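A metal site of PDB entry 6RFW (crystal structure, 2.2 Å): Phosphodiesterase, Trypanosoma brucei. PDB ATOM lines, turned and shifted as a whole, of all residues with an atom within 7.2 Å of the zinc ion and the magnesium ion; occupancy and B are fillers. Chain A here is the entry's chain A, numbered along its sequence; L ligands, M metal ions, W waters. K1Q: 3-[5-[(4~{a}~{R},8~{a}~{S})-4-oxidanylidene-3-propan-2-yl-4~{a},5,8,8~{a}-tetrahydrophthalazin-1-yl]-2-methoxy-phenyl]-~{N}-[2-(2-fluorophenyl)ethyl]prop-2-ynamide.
ND1 of His 151 is in hydrogen-bond range of O of Ala 148, 2.7 Å away.
The side-chain hydroxyl (OH) of Tyr 110 lies close to a ring nitrogen (ND1) of His 115.
Within 4 Å of the zinc ion: His 115, His 151, Asp 152 and Asp 264.
The nearest printed residue that does not touch the zinc ion is His 111 (4.2 Å).
Within 4 Å of the magnesium ion: Asp 152.
The nearest printed residue that does not touch the magnesium ion is His 151 (4.1 Å).
The zinc ion is bound by water W3, at 1.8 Å.
The zinc ion is bound by NE2 of His 151, 2.0 Å away.
The side-chain carboxylate (OD1) of Asp 264 is bound to the zinc ion, 2.1 Å away.
The zinc ion is bound by the side-chain carboxylate (OD2) of Asp 152.
NE2 of His 115 is bound to the zinc ion, at 2.3 Å.
Water W2 is bound to the zinc ion (2.3 Å).
The magnesium ion is bound by water W2.
Water W5 is bound to the magnesium ion (1.9 Å).
Water W1 is bound to the magnesium ion, at 2.0 Å.
OD1 of Asp 152 is bound to the magnesium ion (2.0 Å).
The magnesium ion is bound by water W6 (2.1 Å).
The magnesium ion is bound by water W4 (2.2 Å).
Water W3 lies within hydrogen-bond range of a ring nitrogen (NE2) of His 111 (3.1 Å) and the side-chain carboxylate of Asp 264 (3.2 Å).
Water W5 bridges OG1 of Thr 225 (2.8 Å) and O of His 151 (2.8 Å).
Water W1 bridges a ring nitrogen (NE2) of His 187 and the side-chain carboxylate of Glu 184.
Water W4 lies within hydrogen-bond range of OE2 of Glu 184 and O of Thr 225.
Water W6 bridges a ring nitrogen (NE2) of His 111 (3.1 Å) and a ring nitrogen (NE2) of His 155 (3.4 Å).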
ATOM      1  N   TYR A 110     -21.094  15.216   0.859  1.00  0.00           N
ATOM      2  CA  TYR A 110     -20.198  15.611  -0.268  1.00  0.00           C
ATOM      3  C   TYR A 110     -19.017  14.636  -0.434  1.00  0.00           C
ATOM      4  O   TYR A 110     -18.911  14.014  -1.493  1.00  0.00           O
ATOM      5  CB  TYR A 110     -19.660  17.039  -0.094  1.00  0.00           C
ATOM      6  CG  TYR A 110     -18.833  17.520  -1.259  1.00  0.00           C
ATOM      7  CD1 TYR A 110     -19.409  18.052  -2.398  1.00  0.00           C
ATOM      8  CD2 TYR A 110     -17.441  17.441  -1.234  1.00  0.00           C
ATOM      9  CE1 TYR A 110     -18.661  18.508  -3.460  1.00  0.00           C
ATOM     10  CE2 TYR A 110     -16.675  17.886  -2.300  1.00  0.00           C
ATOM     11  CZ  TYR A 110     -17.282  18.421  -3.419  1.00  0.00           C
ATOM     12  OH  TYR A 110     -16.510  18.870  -4.466  1.00  0.00           O
ATOM     13  N   HIS A 111     -18.183  14.511   0.582  1.00  0.00           N
ATOM     14  CA  HIS A 111     -16.954  13.708   0.549  1.00  0.00           C
ATOM     15  C   HIS A 111     -17.305  12.244   0.709  1.00  0.00           C
ATOM     16  O   HIS A 111     -16.742  11.610   1.606  1.00  0.00           O
ATOM     17  CB  HIS A 111     -15.958  14.189   1.593  1.00  0.00           C
ATOM     18  CG  HIS A 111     -15.395  15.523   1.268  1.00  0.00           C
ATOM     19  ND1 HIS A 111     -15.631  16.616   2.053  1.00  0.00           N
ATOM     20  CD2 HIS A 111     -14.615  15.953   0.243  1.00  0.00           C
ATOM     21  CE1 HIS A 111     -14.999  17.663   1.560  1.00  0.00           C
ATOM     22  NE2 HIS A 111     -14.362  17.287   0.434  1.00  0.00           N
ATOM     23  N   HIS A 115     -18.209  11.582  -4.888  1.00  0.00           N
ATOM     24  CA  HIS A 115     -17.244  12.673  -5.085  1.00  0.00           C
ATOM     25  C   HIS A 115     -15.991  12.151  -5.783  1.00  0.00           C
ATOM     26  O   HIS A 115     -15.520  12.837  -6.690  1.00  0.00           O
ATOM     27  CB  HIS A 115     -16.922  13.385  -3.789  1.00  0.00           C
ATOM     28  CG  HIS A 115     -15.754  14.319  -3.911  1.00  0.00           C
ATOM     29  ND1 HIS A 115     -15.819  15.486  -4.644  1.00  0.00           N
ATOM     30  CD2 HIS A 115     -14.503  14.237  -3.420  1.00  0.00           C
ATOM     31  CE1 HIS A 115     -14.670  16.103  -4.562  1.00  0.00           C
ATOM     32  NE2 HIS A 115     -13.856  15.365  -3.816  1.00  0.00           N
ATOM     33  N   VAL A 116     -15.455  11.015  -5.398  1.00  0.00           N
ATOM     34  CA  VAL A 116     -14.096  10.594  -5.872  1.00  0.00           C
ATOM     35  C   VAL A 116     -14.237   9.923  -7.240  1.00  0.00           C
ATOM     36  O   VAL A 116     -13.284   9.967  -8.030  1.00  0.00           O
ATOM     37  CB  VAL A 116     -13.357   9.717  -4.854  1.00  0.00           C
ATOM     38  CG1 VAL A 116     -13.262  10.395  -3.494  1.00  0.00           C
ATOM     39  CG2 VAL A 116     -13.994   8.347  -4.701  1.00  0.00           C
ATOM     40  N   VAL A 119     -14.268  12.832  -9.448  1.00  0.00           N
ATOM     41  CA  VAL A 119     -12.891  13.365  -9.630  1.00  0.00           C
ATOM     42  C   VAL A 119     -12.150  12.477 -10.637  1.00  0.00           C
ATOM     43  O   VAL A 119     -11.485  13.037 -11.535  1.00  0.00           O
ATOM     44  CB  VAL A 119     -12.133  13.501  -8.291  1.00  0.00           C
ATOM     45  CG1 VAL A 119     -10.649  13.807  -8.494  1.00  0.00           C
ATOM     46  CG2 VAL A 119     -12.766  14.572  -7.415  1.00  0.00           C
ATOM     47  N   ALA A 148      -7.360   9.342  -7.925  1.00  0.00           N
ATOM     48  CA  ALA A 148      -8.695   9.975  -7.828  1.00  0.00           C
ATOM     49  C   ALA A 148      -9.556   9.213  -6.801  1.00  0.00           C
ATOM     50  O   ALA A 148     -10.143   9.842  -5.930  1.00  0.00           O
ATOM     51  CB  ALA A 148      -9.334   9.995  -9.190  1.00  0.00           C
ATOM     52  N   HIS A 151      -8.363   9.456  -2.812  1.00  0.00           N
ATOM     53  CA  HIS A 151      -7.823  10.769  -2.353  1.00  0.00           C
ATOM     54  C   HIS A 151      -8.626  11.384  -1.181  1.00  0.00           C
ATOM     55  O   HIS A 151      -8.157  12.372  -0.564  1.00  0.00           O
ATOM     56  CB  HIS A 151      -7.719  11.732  -3.553  1.00  0.00           C
ATOM     57  CG  HIS A 151      -8.948  12.546  -3.745  1.00  0.00           C
ATOM     58  ND1 HIS A 151     -10.007  12.122  -4.526  1.00  0.00           N
ATOM     59  CD2 HIS A 151      -9.296  13.745  -3.222  1.00  0.00           C
ATOM     60  CE1 HIS A 151     -10.954  13.041  -4.482  1.00  0.00           C
ATOM     61  NE2 HIS A 151     -10.550  14.049  -3.691  1.00  0.00           N
ATOM     62  N   ASP A 152      -9.806  10.856  -0.846  1.00  0.00           N
ATOM     63  CA  ASP A 152     -10.567  11.332   0.340  1.00  0.00           C
ATOM     64  C   ASP A 152     -10.982  10.152   1.250  1.00  0.00           C
ATOM     65  O   ASP A 152     -11.941  10.315   2.003  1.00  0.00           O
ATOM     66  CB  ASP A 152     -11.783  12.141  -0.098  1.00  0.00           C
ATOM     67  CG  ASP A 152     -11.498  13.598  -0.428  1.00  0.00           C
ATOM     68  OD1 ASP A 152     -10.636  14.229   0.245  1.00  0.00           O
ATOM     69  OD2 ASP A 152     -12.175  14.091  -1.328  1.00  0.00           O
ATOM     70  N   LEU A 153     -10.283   9.020   1.193  1.00  0.00           N
ATOM     71  CA  LEU A 153     -10.695   7.781   1.933  1.00  0.00           C
ATOM     72  C   LEU A 153     -11.003   8.069   3.391  1.00  0.00           C
ATOM     73  O   LEU A 153     -10.147   8.627   4.091  1.00  0.00           O
ATOM     74  CB  LEU A 153      -9.594   6.722   1.870  1.00  0.00           C
ATOM     75  CG  LEU A 153      -9.513   5.988   0.554  1.00  0.00           C
ATOM     76  CD1 LEU A 153      -8.174   5.287   0.426  1.00  0.00           C
ATOM     77  CD2 LEU A 153     -10.668   5.002   0.417  1.00  0.00           C
ATOM     78  N   HIS A 155     -13.212   9.944   4.816  1.00  0.00           N
ATOM     79  CA  HIS A 155     -13.525  11.363   5.149  1.00  0.00           C
ATOM     80  C   HIS A 155     -14.841  11.388   5.950  1.00  0.00           C
ATOM     81  O   HIS A 155     -15.772  10.645   5.573  1.00  0.00           O
ATOM     82  CB  HIS A 155     -13.579  12.169   3.846  1.00  0.00           C
ATOM     83  CG  HIS A 155     -13.421  13.633   4.030  1.00  0.00           C
ATOM     84  ND1 HIS A 155     -14.294  14.367   4.787  1.00  0.00           N
ATOM     85  CD2 HIS A 155     -12.510  14.500   3.520  1.00  0.00           C
ATOM     86  CE1 HIS A 155     -13.913  15.649   4.758  1.00  0.00           C
ATOM     87  NE2 HIS A 155     -12.815  15.760   3.965  1.00  0.00           N
ATOM     88  N   LEU A 183      -6.256  15.135   7.498  1.00  0.00           N
ATOM     89  CA  LEU A 183      -7.072  14.214   6.653  1.00  0.00           C
ATOM     90  C   LEU A 183      -6.193  13.611   5.563  1.00  0.00           C
ATOM     91  O   LEU A 183      -6.320  12.401   5.289  1.00  0.00           O
ATOM     92  CB  LEU A 183      -8.230  14.975   6.016  1.00  0.00           C
ATOM     93  CG  LEU A 183      -9.401  15.337   6.942  1.00  0.00           C
ATOM     94  CD1 LEU A 183     -10.171  16.539   6.392  1.00  0.00           C
ATOM     95  CD2 LEU A 183     -10.328  14.154   7.125  1.00  0.00           C
ATOM     96  N   GLU A 184      -5.327  14.402   4.953  1.00  0.00           N
ATOM     97  CA  GLU A 184      -4.633  13.943   3.720  1.00  0.00           C
ATOM     98  C   GLU A 184      -3.739  12.769   4.101  1.00  0.00           C
ATOM     99  O   GLU A 184      -3.752  11.769   3.362  1.00  0.00           O
ATOM    100  CB  GLU A 184      -3.871  15.069   3.025  1.00  0.00           C
ATOM    101  CG  GLU A 184      -4.795  16.128   2.431  1.00  0.00           C
ATOM    102  CD  GLU A 184      -5.528  17.068   3.383  1.00  0.00           C
ATOM    103  OE1 GLU A 184      -5.042  17.281   4.512  1.00  0.00           O
ATOM    104  OE2 GLU A 184      -6.589  17.573   2.987  1.00  0.00           O
ATOM    105  N   HIS A 187      -5.776   9.652   4.557  1.00  0.00           N
ATOM    106  CA  HIS A 187      -6.194   9.116   3.235  1.00  0.00           C
ATOM    107  C   HIS A 187      -5.070   8.245   2.726  1.00  0.00           C
ATOM    108  O   HIS A 187      -5.335   7.102   2.312  1.00  0.00           O
ATOM    109  CB  HIS A 187      -6.569  10.219   2.225  1.00  0.00           C
ATOM    110  CG  HIS A 187      -7.616  11.162   2.697  1.00  0.00           C
ATOM    111  ND1 HIS A 187      -8.690  10.748   3.487  1.00  0.00           N
ATOM    112  CD2 HIS A 187      -7.749  12.501   2.535  1.00  0.00           C
ATOM    113  CE1 HIS A 187      -9.440  11.802   3.786  1.00  0.00           C
ATOM    114  NE2 HIS A 187      -8.896  12.900   3.215  1.00  0.00           N
ATOM    115  N   VAL A 222      -2.085  13.210  -3.273  1.00  0.00           N
ATOM    116  CA  VAL A 222      -3.121  13.280  -2.182  1.00  0.00           C
ATOM    117  C   VAL A 222      -2.770  14.386  -1.192  1.00  0.00           C
ATOM    118  O   VAL A 222      -3.685  15.139  -0.808  1.00  0.00           O
ATOM    119  CB  VAL A 222      -3.237  11.954  -1.429  1.00  0.00           C
ATOM    120  CG1 VAL A 222      -4.311  12.084  -0.339  1.00  0.00           C
ATOM    121  CG2 VAL A 222      -3.528  10.828  -2.391  1.00  0.00           C
ATOM    122  N   THR A 225      -3.728  17.880  -2.154  1.00  0.00           N
ATOM    123  CA  THR A 225      -5.182  18.226  -2.201  1.00  0.00           C
ATOM    124  C   THR A 225      -5.560  19.093  -1.012  1.00  0.00           C
ATOM    125  O   THR A 225      -6.707  19.618  -1.014  1.00  0.00           O
ATOM    126  CB  THR A 225      -6.077  16.990  -2.261  1.00  0.00           C
ATOM    127  OG1 THR A 225      -5.924  16.138  -1.117  1.00  0.00           O
ATOM    128  CG2 THR A 225      -5.782  16.224  -3.530  1.00  0.00           C
ATOM    129  N   ASP A 226      -4.662  19.219  -0.010  1.00  0.00           N
ATOM    130  CA  ASP A 226      -4.863  20.125   1.151  1.00  0.00           C
ATOM    131  C   ASP A 226      -4.870  21.576   0.676  1.00  0.00           C
ATOM    132  O   ASP A 226      -3.810  22.042   0.261  1.00  0.00           O
ATOM    133  CB  ASP A 226      -3.753  19.959   2.199  1.00  0.00           C
ATOM    134  CG  ASP A 226      -3.962  20.743   3.491  1.00  0.00           C
ATOM    135  OD1 ASP A 226      -4.668  21.787   3.492  1.00  0.00           O
ATOM    136  OD2 ASP A 226      -3.446  20.280   4.497  1.00  0.00           O
ATOM    137  N   LEU A 260      -4.847  16.530 -10.133  1.00  0.00           N
ATOM    138  CA  LEU A 260      -5.724  16.017  -9.043  1.00  0.00           C
ATOM    139  C   LEU A 260      -6.364  17.213  -8.359  1.00  0.00           C
ATOM    140  O   LEU A 260      -7.583  17.176  -8.169  1.00  0.00           O
ATOM    141  CB  LEU A 260      -4.963  15.153  -8.045  1.00  0.00           C
ATOM    142  CG  LEU A 260      -5.822  14.546  -6.932  1.00  0.00           C
ATOM    143  CD1 LEU A 260      -6.745  13.489  -7.485  1.00  0.00           C
ATOM    144  CD2 LEU A 260      -4.975  13.935  -5.859  1.00  0.00           C
ATOM    145  N   GLY A 263      -9.186  18.452 -10.618  1.00  0.00           N
ATOM    146  CA  GLY A 263     -10.355  17.565 -10.461  1.00  0.00           C
ATOM    147  C   GLY A 263     -11.117  17.900  -9.185  1.00  0.00           C
ATOM    148  O   GLY A 263     -12.328  17.950  -9.205  1.00  0.00           O
ATOM    149  N   ASP A 264     -10.398  18.116  -8.093  1.00  0.00           N
ATOM    150  CA  ASP A 264     -10.993  18.261  -6.756  1.00  0.00           C
ATOM    151  C   ASP A 264     -11.772  19.579  -6.647  1.00  0.00           C
ATOM    152  O   ASP A 264     -12.651  19.651  -5.805  1.00  0.00           O
ATOM    153  CB  ASP A 264      -9.898  18.157  -5.683  1.00  0.00           C
ATOM    154  CG  ASP A 264     -10.394  17.670  -4.330  1.00  0.00           C
ATOM    155  OD1 ASP A 264     -11.358  16.920  -4.314  1.00  0.00           O
ATOM    156  OD2 ASP A 264      -9.771  18.038  -3.302  1.00  0.00           O
ATOM    157  N   ILE A 265     -11.464  20.612  -7.433  1.00  0.00           N
ATOM    158  CA  ILE A 265     -12.273  21.863  -7.462  1.00  0.00           C
ATOM    159  C   ILE A 265     -12.940  22.066  -8.829  1.00  0.00           C
ATOM    160  O   ILE A 265     -13.182  23.220  -9.199  1.00  0.00           O
ATOM    161  CB  ILE A 265     -11.411  23.058  -7.033  1.00  0.00           C
ATOM    162  CG1 ILE A 265     -10.311  23.392  -8.029  1.00  0.00           C
ATOM    163  CG2 ILE A 265     -10.827  22.804  -5.642  1.00  0.00           C
ATOM    164  CD1 ILE A 265      -9.548  24.631  -7.653  1.00  0.00           C
HETATM  165  C6  K1Q L   1     -15.282  22.849  -3.010  1.00  0.00           C
HETATM  166  C5  K1Q L   1     -14.999  23.724  -1.956  1.00  0.00           C
HETATM  167  C8  K1Q L   1     -13.814  23.521  -1.082  1.00  0.00           C
HETATM  168  C4  K1Q L   1     -15.846  24.812  -1.720  1.00  0.00           C
HETATM  169  N3  K1Q L   1     -19.362  28.629  -0.528  1.00  0.00           N
HETATM  170  C2  K1Q L   1     -17.236  24.141  -3.575  1.00  0.00           C
HETATM  171  N1  K1Q L   1     -13.419  24.546  -0.408  1.00  0.00           N
HETATM  172  C1  K1Q L   1     -18.869  23.403  -5.187  1.00  0.00           C
HETATM  173  C10 K1Q L   1     -12.427  26.291   1.934  1.00  0.00           C
HETATM  174  C11 K1Q L   1     -11.560  26.614  -0.421  1.00  0.00           C
HETATM  175  C12 K1Q L   1     -11.882  23.188   0.887  1.00  0.00           C
HETATM  176  C13 K1Q L   1     -12.648  21.947   0.471  1.00  0.00           C
HETATM  177  C14 K1Q L   1     -11.883  20.622   0.643  1.00  0.00           C
HETATM  178  C15 K1Q L   1     -10.943  20.339  -0.484  1.00  0.00           C
HETATM  179  C16 K1Q L   1     -11.024  20.929  -1.664  1.00  0.00           C
HETATM  180  C17 K1Q L   1     -11.985  22.026  -1.990  1.00  0.00           C
HETATM  181  C18 K1Q L   1     -13.139  22.152  -0.981  1.00  0.00           C
HETATM  182  C19 K1Q L   1     -17.876  26.128  -2.256  1.00  0.00           C
HETATM  183  C20 K1Q L   1     -18.712  26.964  -2.007  1.00  0.00           C
HETATM  184  C21 K1Q L   1     -19.706  27.904  -1.593  1.00  0.00           C
HETATM  185  C22 K1Q L   1     -18.353  28.189   0.411  1.00  0.00           C
HETATM  186  C23 K1Q L   1     -17.631  29.345   1.016  1.00  0.00           C
HETATM  187  C24 K1Q L   1     -16.661  30.128   0.164  1.00  0.00           C
HETATM  188  C25 K1Q L   1     -15.403  29.647  -0.193  1.00  0.00           C
HETATM  189  C26 K1Q L   1     -14.480  30.379  -0.903  1.00  0.00           C
HETATM  190  C27 K1Q L   1     -14.814  31.663  -1.271  1.00  0.00           C
HETATM  191  C28 K1Q L   1     -16.042  32.187  -0.930  1.00  0.00           C
HETATM  192  C29 K1Q L   1     -16.963  31.433  -0.216  1.00  0.00           C
HETATM  193  C3  K1Q L   1     -16.968  25.042  -2.522  1.00  0.00           C
HETATM  194  C7  K1Q L   1     -16.386  23.066  -3.815  1.00  0.00           C
HETATM  195  C9  K1Q L   1     -11.666  25.673   0.776  1.00  0.00           C
HETATM  196  F1  K1Q L   1     -15.058  28.380   0.168  1.00  0.00           F
HETATM  197  N2  K1Q L   1     -12.336  24.398   0.390  1.00  0.00           N
HETATM  198  O1  K1Q L   1     -18.354  24.421  -4.324  1.00  0.00           O
HETATM  199  O2  K1Q L   1     -10.895  23.156   1.597  1.00  0.00           O
HETATM  200  O3  K1Q L   1     -20.805  28.021  -2.147  1.00  0.00           O
HETATM  201 ZN    ZN M   1     -11.760  15.480  -2.860  1.00  0.00          ZN
HETATM  202 MG    MG M   2      -9.730  16.026   0.504  1.00  0.00          MG
HETATM  203  O   HOH W   1      -9.275  15.813   2.456  1.00  0.00           O
HETATM  204  O   HOH W   2     -10.173  16.212  -1.308  1.00  0.00           O
HETATM  205  O   HOH W   3     -12.320  16.868  -1.844  1.00  0.00           O
HETATM  206  O   HOH W   4      -8.220  17.620   0.537  1.00  0.00           O
HETATM  207  O   HOH W   5      -8.174  15.058   0.055  1.00  0.00           O
HETATM  208  O   HOH W   6     -11.377  17.068   1.146  1.00  0.00           O
